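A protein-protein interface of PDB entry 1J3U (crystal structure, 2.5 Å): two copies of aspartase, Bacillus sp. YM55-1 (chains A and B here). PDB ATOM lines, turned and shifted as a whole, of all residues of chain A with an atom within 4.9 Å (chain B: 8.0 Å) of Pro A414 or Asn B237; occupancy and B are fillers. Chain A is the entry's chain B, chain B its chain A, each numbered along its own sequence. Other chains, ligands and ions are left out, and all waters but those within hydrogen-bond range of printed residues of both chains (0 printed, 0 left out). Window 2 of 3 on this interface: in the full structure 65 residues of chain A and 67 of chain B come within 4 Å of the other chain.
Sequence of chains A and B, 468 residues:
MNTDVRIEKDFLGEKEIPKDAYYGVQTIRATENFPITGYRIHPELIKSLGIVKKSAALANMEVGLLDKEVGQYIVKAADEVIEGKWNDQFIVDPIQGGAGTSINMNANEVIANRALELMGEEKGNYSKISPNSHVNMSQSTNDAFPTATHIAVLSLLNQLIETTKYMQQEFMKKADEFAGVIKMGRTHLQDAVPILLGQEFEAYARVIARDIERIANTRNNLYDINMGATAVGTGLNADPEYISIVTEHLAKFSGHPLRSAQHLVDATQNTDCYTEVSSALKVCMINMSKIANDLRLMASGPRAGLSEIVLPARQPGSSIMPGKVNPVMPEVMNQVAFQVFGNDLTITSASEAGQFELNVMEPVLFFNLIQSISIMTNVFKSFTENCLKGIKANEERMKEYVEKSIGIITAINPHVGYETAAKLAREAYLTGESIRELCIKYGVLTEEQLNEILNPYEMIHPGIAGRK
The backbone carbonyl oxygen (O) of Thr A410 lies within hydrogen-bond range of the side-chain amide nitrogen (ND2) of Asn B237, 2.9 Å away.
The backbone carbonyl oxygen of Ala B238 lies within hydrogen-bond range of the backbone NH of Gly A463, at 3.1 Å.
The backbone NH of Leu B236 lies close to the side-chain hydroxyl of Thr B234 (3.5 Å).
Among the printed residues, pairs that only touch across the chains: Pro A414 with Asn B237 (3.0 Å), His A461 with Thr B234 (3.1 Å), Thr A410 with Leu B236 (3.3 Å) and Gly A463 with Asn B237 (3.5 Å).
Asn B237 touches three residues of chain A.
No residue of chain B comes within 4 Å of Asn A413.
Of the printed residues of chain A, Thr B234 touches His A461 (3.1 Å).
Printed residues of chain B within 4 Å of His A461: Thr B234.
Printed residues of chain B within 4 Å of Thr A410: Leu B236 and Asn B237.
Of the printed residues of chain A, Leu B236 touches Thr A410 (3.3 Å).
Thr B230 touches none of the printed residues of chain A.
Ile B243 touches none of the printed residues of chain A.
The nearest residue of chain B that does not touch Pro A414 is Leu B236 (6.8 Å).
The nearest residue of chain A that does not touch Asn B237 is Ala A411 (4.5 Å).
The nearest printed residue of chain B that does not touch Gly A463 is Pro B240 (4.1 Å).
Hydrophobic or aromatic side chains of chain B within 4 Å of the printed part of chain A: Leu B236.
Along chain B the printed residues that touch a printed residue of chain A span positions 234 to 238.
No position is printed for both chains.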
ATOM      1  N   ILE A 409      25.022  25.144  11.525  1.00  0.00           N
ATOM      2  CA  ILE A 409      25.509  24.334  12.641  1.00  0.00           C
ATOM      3  C   ILE A 409      24.589  24.457  13.844  1.00  0.00           C
ATOM      4  O   ILE A 409      24.379  23.486  14.567  1.00  0.00           O
ATOM      5  CB  ILE A 409      26.937  24.770  13.084  1.00  0.00           C
ATOM      6  CG1 ILE A 409      27.521  23.763  14.087  1.00  0.00           C
ATOM      7  CG2 ILE A 409      26.886  26.151  13.732  1.00  0.00           C
ATOM      8  CD1 ILE A 409      27.828  22.405  13.495  1.00  0.00           C
ATOM      9  N   THR A 410      24.049  25.654  14.057  1.00  0.00           N
ATOM     10  CA  THR A 410      23.151  25.908  15.182  1.00  0.00           C
ATOM     11  C   THR A 410      21.977  24.924  15.171  1.00  0.00           C
ATOM     12  O   THR A 410      21.533  24.461  16.219  1.00  0.00           O
ATOM     13  CB  THR A 410      22.606  27.369  15.152  1.00  0.00           C
ATOM     14  OG1 THR A 410      23.701  28.294  15.210  1.00  0.00           O
ATOM     15  CG2 THR A 410      21.694  27.628  16.337  1.00  0.00           C
ATOM     16  N   ALA A 411      21.486  24.598  13.984  1.00  0.00           N
ATOM     17  CA  ALA A 411      20.375  23.669  13.869  1.00  0.00           C
ATOM     18  C   ALA A 411      20.843  22.283  14.282  1.00  0.00           C
ATOM     19  O   ALA A 411      20.167  21.582  15.038  1.00  0.00           O
ATOM     20  CB  ALA A 411      19.864  23.645  12.439  1.00  0.00           C
ATOM     21  N   ILE A 412      22.023  21.914  13.785  1.00  0.00           N
ATOM     22  CA  ILE A 412      22.647  20.616  14.033  1.00  0.00           C
ATOM     23  C   ILE A 412      23.210  20.456  15.447  1.00  0.00           C
ATOM     24  O   ILE A 412      23.110  19.388  16.046  1.00  0.00           O
ATOM     25  CB  ILE A 412      23.776  20.384  13.007  1.00  0.00           C
ATOM     26  CG1 ILE A 412      23.180  20.313  11.602  1.00  0.00           C
ATOM     27  CG2 ILE A 412      24.545  19.124  13.337  1.00  0.00           C
ATOM     28  CD1 ILE A 412      24.212  20.358  10.506  1.00  0.00           C
ATOM     29  N   ASN A 413      23.801  21.521  15.972  1.00  0.00           N
ATOM     30  CA  ASN A 413      24.385  21.508  17.307  1.00  0.00           C
ATOM     31  C   ASN A 413      23.638  20.679  18.357  1.00  0.00           C
ATOM     32  O   ASN A 413      24.233  19.841  19.034  1.00  0.00           O
ATOM     33  CB  ASN A 413      24.531  22.938  17.826  1.00  0.00           C
ATOM     34  CG  ASN A 413      24.578  22.998  19.337  1.00  0.00           C
ATOM     35  OD1 ASN A 413      25.565  22.601  19.957  1.00  0.00           O
ATOM     36  ND2 ASN A 413      23.497  23.478  19.946  1.00  0.00           N
ATOM     37  N   PRO A 414      22.327  20.913  18.520  1.00  0.00           N
ATOM     38  CA  PRO A 414      21.542  20.167  19.507  1.00  0.00           C
ATOM     39  C   PRO A 414      21.632  18.655  19.360  1.00  0.00           C
ATOM     40  O   PRO A 414      21.550  17.932  20.348  1.00  0.00           O
ATOM     41  CB  PRO A 414      20.124  20.673  19.271  1.00  0.00           C
ATOM     42  CG  PRO A 414      20.348  22.070  18.812  1.00  0.00           C
ATOM     43  CD  PRO A 414      21.481  21.898  17.830  1.00  0.00           C
ATOM     44  N   HIS A 415      21.799  18.175  18.132  1.00  0.00           N
ATOM     45  CA  HIS A 415      21.882  16.737  17.899  1.00  0.00           C
ATOM     46  C   HIS A 415      23.301  16.196  17.924  1.00  0.00           C
ATOM     47  O   HIS A 415      23.528  15.058  17.526  1.00  0.00           O
ATOM     48  CB  HIS A 415      21.251  16.372  16.551  1.00  0.00           C
ATOM     49  CG  HIS A 415      19.861  16.903  16.366  1.00  0.00           C
ATOM     50  ND1 HIS A 415      19.608  18.144  15.830  1.00  0.00           N
ATOM     51  CD2 HIS A 415      18.659  16.361  16.660  1.00  0.00           C
ATOM     52  CE1 HIS A 415      18.301  18.349  15.801  1.00  0.00           C
ATOM     53  NE2 HIS A 415      17.701  17.281  16.300  1.00  0.00           N
ATOM     54  N   VAL A 416      24.258  16.991  18.385  1.00  0.00           N
ATOM     55  CA  VAL A 416      25.649  16.543  18.403  1.00  0.00           C
ATOM     56  C   VAL A 416      26.464  17.100  19.573  1.00  0.00           C
ATOM     57  O   VAL A 416      27.602  16.683  19.788  1.00  0.00           O
ATOM     58  CB  VAL A 416      26.367  16.925  17.072  1.00  0.00           C
ATOM     59  CG1 VAL A 416      27.743  16.298  17.018  1.00  0.00           C
ATOM     60  CG2 VAL A 416      25.546  16.468  15.875  1.00  0.00           C
ATOM     61  N   GLY A 417      25.884  18.038  20.322  1.00  0.00           N
ATOM     62  CA  GLY A 417      26.592  18.630  21.448  1.00  0.00           C
ATOM     63  C   GLY A 417      27.560  19.720  21.017  1.00  0.00           C
ATOM     64  O   GLY A 417      28.151  19.637  19.941  1.00  0.00           O
ATOM     65  N   HIS A 461      11.893  28.206  13.377  1.00  0.00           N
ATOM     66  CA  HIS A 461      10.899  28.494  14.403  1.00  0.00           C
ATOM     67  C   HIS A 461      11.354  27.964  15.757  1.00  0.00           C
ATOM     68  O   HIS A 461      12.105  26.986  15.837  1.00  0.00           O
ATOM     69  CB  HIS A 461       9.563  27.866  14.009  1.00  0.00           C
ATOM     70  CG  HIS A 461       8.923  28.517  12.823  1.00  0.00           C
ATOM     71  ND1 HIS A 461       8.224  29.703  12.909  1.00  0.00           N
ATOM     72  CD2 HIS A 461       8.893  28.160  11.516  1.00  0.00           C
ATOM     73  CE1 HIS A 461       7.789  30.046  11.711  1.00  0.00           C
ATOM     74  NE2 HIS A 461       8.181  29.125  10.846  1.00  0.00           N
ATOM     75  N   GLY A 463      11.552  26.038  19.288  1.00  0.00           N
ATOM     76  CA  GLY A 463      11.136  24.713  19.695  1.00  0.00           C
ATOM     77  C   GLY A 463      12.220  23.988  20.466  1.00  0.00           C
ATOM     78  O   GLY A 463      13.361  24.443  20.522  1.00  0.00           O
ATOM     79  N   ALA A 465      14.713  20.615  21.223  1.00  0.00           N
ATOM     80  CA  ALA A 465      15.719  20.060  20.320  1.00  0.00           C
ATOM     81  C   ALA A 465      15.249  18.791  19.608  1.00  0.00           C
ATOM     82  O   ALA A 465      15.953  18.262  18.749  1.00  0.00           O
ATOM     83  CB  ALA A 465      16.999  19.778  21.086  1.00  0.00           C
ATOM     84  N   LEU B  65      17.552  24.995  32.695  1.00  0.00           N
ATOM     85  CA  LEU B  65      18.739  25.276  31.893  1.00  0.00           C
ATOM     86  C   LEU B  65      19.893  25.855  32.703  1.00  0.00           C
ATOM     87  O   LEU B  65      21.059  25.691  32.342  1.00  0.00           O
ATOM     88  CB  LEU B  65      18.393  26.238  30.759  1.00  0.00           C
ATOM     89  CG  LEU B  65      17.553  25.599  29.662  1.00  0.00           C
ATOM     90  CD1 LEU B  65      17.312  26.588  28.534  1.00  0.00           C
ATOM     91  CD2 LEU B  65      18.280  24.383  29.145  1.00  0.00           C
ATOM     92  N   SER B 138      20.495  31.541  27.063  1.00  0.00           N
ATOM     93  CA  SER B 138      19.208  31.565  26.357  1.00  0.00           C
ATOM     94  C   SER B 138      18.798  32.885  25.714  1.00  0.00           C
ATOM     95  O   SER B 138      17.631  33.064  25.359  1.00  0.00           O
ATOM     96  CB  SER B 138      18.088  31.093  27.294  1.00  0.00           C
ATOM     97  OG  SER B 138      18.380  29.808  27.821  1.00  0.00           O
ATOM     98  N   GLY B 228      13.709  36.257  23.339  1.00  0.00           N
ATOM     99  CA  GLY B 228      13.679  34.874  22.909  1.00  0.00           C
ATOM    100  C   GLY B 228      13.676  34.761  21.404  1.00  0.00           C
ATOM    101  O   GLY B 228      13.234  33.758  20.847  1.00  0.00           O
ATOM    102  N   THR B 230      16.492  35.137  19.758  1.00  0.00           N
ATOM    103  CA  THR B 230      17.843  34.677  19.463  1.00  0.00           C
ATOM    104  C   THR B 230      18.503  35.611  18.449  1.00  0.00           C
ATOM    105  O   THR B 230      18.258  36.820  18.455  1.00  0.00           O
ATOM    106  CB  THR B 230      17.885  33.197  18.940  1.00  0.00           C
ATOM    107  OG1 THR B 230      17.040  33.039  17.792  1.00  0.00           O
ATOM    108  CG2 THR B 230      17.447  32.238  20.033  1.00  0.00           C
ATOM    109  N   THR B 234      14.253  33.881  14.741  1.00  0.00           N
ATOM    110  CA  THR B 234      13.634  32.594  14.447  1.00  0.00           C
ATOM    111  C   THR B 234      13.405  31.788  15.731  1.00  0.00           C
ATOM    112  O   THR B 234      12.649  30.813  15.727  1.00  0.00           O
ATOM    113  CB  THR B 234      14.515  31.756  13.485  1.00  0.00           C
ATOM    114  OG1 THR B 234      15.821  31.603  14.047  1.00  0.00           O
ATOM    115  CG2 THR B 234      14.644  32.434  12.131  1.00  0.00           C
ATOM    116  N   GLY B 235      14.055  32.197  16.821  1.00  0.00           N
ATOM    117  CA  GLY B 235      13.908  31.492  18.085  1.00  0.00           C
ATOM    118  C   GLY B 235      14.543  30.115  18.051  1.00  0.00           C
ATOM    119  O   GLY B 235      14.326  29.300  18.941  1.00  0.00           O
ATOM    120  N   LEU B 236      15.330  29.861  17.010  1.00  0.00           N
ATOM    121  CA  LEU B 236      16.018  28.588  16.810  1.00  0.00           C
ATOM    122  C   LEU B 236      16.608  28.008  18.096  1.00  0.00           C
ATOM    123  O   LEU B 236      17.531  28.581  18.693  1.00  0.00           O
ATOM    124  CB  LEU B 236      17.128  28.772  15.775  1.00  0.00           C
ATOM    125  CG  LEU B 236      17.973  27.556  15.399  1.00  0.00           C
ATOM    126  CD1 LEU B 236      17.081  26.454  14.849  1.00  0.00           C
ATOM    127  CD2 LEU B 236      19.020  27.980  14.371  1.00  0.00           C
ATOM    128  N   ASN B 237      16.067  26.861  18.504  1.00  0.00           N
ATOM    129  CA  ASN B 237      16.494  26.147  19.712  1.00  0.00           C
ATOM    130  C   ASN B 237      15.985  26.741  21.019  1.00  0.00           C
ATOM    131  O   ASN B 237      16.169  26.140  22.077  1.00  0.00           O
ATOM    132  CB  ASN B 237      18.020  26.037  19.765  1.00  0.00           C
ATOM    133  CG  ASN B 237      18.574  25.163  18.656  1.00  0.00           C
ATOM    134  OD1 ASN B 237      18.092  24.049  18.433  1.00  0.00           O
ATOM    135  ND2 ASN B 237      19.590  25.661  17.956  1.00  0.00           N
ATOM    136  N   ALA B 238      15.351  27.912  20.954  1.00  0.00           N
ATOM    137  CA  ALA B 238      14.800  28.548  22.150  1.00  0.00           C
ATOM    138  C   ALA B 238      13.584  27.759  22.612  1.00  0.00           C
ATOM    139  O   ALA B 238      12.807  27.278  21.792  1.00  0.00           O
ATOM    140  CB  ALA B 238      14.395  29.984  21.846  1.00  0.00           C
ATOM    141  N   ASP B 239      13.423  27.624  23.922  1.00  0.00           N
ATOM    142  CA  ASP B 239      12.285  26.897  24.488  1.00  0.00           C
ATOM    143  C   ASP B 239      11.085  27.819  24.713  1.00  0.00           C
ATOM    144  O   ASP B 239      11.179  28.801  25.460  1.00  0.00           O
ATOM    145  CB  ASP B 239      12.676  26.265  25.820  1.00  0.00           C
ATOM    146  CG  ASP B 239      11.496  25.637  26.537  1.00  0.00           C
ATOM    147  OD1 ASP B 239      11.666  25.268  27.719  1.00  0.00           O
ATOM    148  OD2 ASP B 239      10.410  25.505  25.924  1.00  0.00           O
ATOM    149  N   PRO B 240       9.940  27.502  24.082  1.00  0.00           N
ATOM    150  CA  PRO B 240       8.724  28.305  24.214  1.00  0.00           C
ATOM    151  C   PRO B 240       8.309  28.567  25.662  1.00  0.00           C
ATOM    152  O   PRO B 240       7.666  29.580  25.950  1.00  0.00           O
ATOM    153  CB  PRO B 240       7.692  27.484  23.440  1.00  0.00           C
ATOM    154  CG  PRO B 240       8.506  26.881  22.364  1.00  0.00           C
ATOM    155  CD  PRO B 240       9.719  26.405  23.125  1.00  0.00           C
ATOM    156  N   TYR B 242      10.469  28.931  28.055  1.00  0.00           N
ATOM    157  CA  TYR B 242      11.442  29.916  28.518  1.00  0.00           C
ATOM    158  C   TYR B 242      10.901  31.296  28.149  1.00  0.00           C
ATOM    159  O   TYR B 242      10.828  32.202  28.987  1.00  0.00           O
ATOM    160  CB  TYR B 242      12.792  29.710  27.828  1.00  0.00           C
ATOM    161  CG  TYR B 242      13.663  30.950  27.844  1.00  0.00           C
ATOM    162  CD1 TYR B 242      14.397  31.307  28.974  1.00  0.00           C
ATOM    163  CD2 TYR B 242      13.690  31.807  26.746  1.00  0.00           C
ATOM    164  CE1 TYR B 242      15.132  32.494  29.007  1.00  0.00           C
ATOM    165  CE2 TYR B 242      14.415  32.993  26.768  1.00  0.00           C
ATOM    166  CZ  TYR B 242      15.131  33.332  27.898  1.00  0.00           C
ATOM    167  OH  TYR B 242      15.813  34.529  27.909  1.00  0.00           O
ATOM    168  N   ILE B 243      10.536  31.441  26.876  1.00  0.00           N
ATOM    169  CA  ILE B 243       9.993  32.688  26.361  1.00  0.00           C
ATOM    170  C   ILE B 243       8.801  33.080  27.216  1.00  0.00           C
ATOM    171  O   ILE B 243       8.799  34.116  27.886  1.00  0.00           O
ATOM    172  CB  ILE B 243       9.527  32.527  24.908  1.00  0.00           C
ATOM    173  CG1 ILE B 243      10.714  32.150  24.021  1.00  0.00           C
ATOM    174  CG2 ILE B 243       8.879  33.821  24.426  1.00  0.00           C
ATOM    175  CD1 ILE B 243      10.372  32.019  22.554  1.00  0.00           C
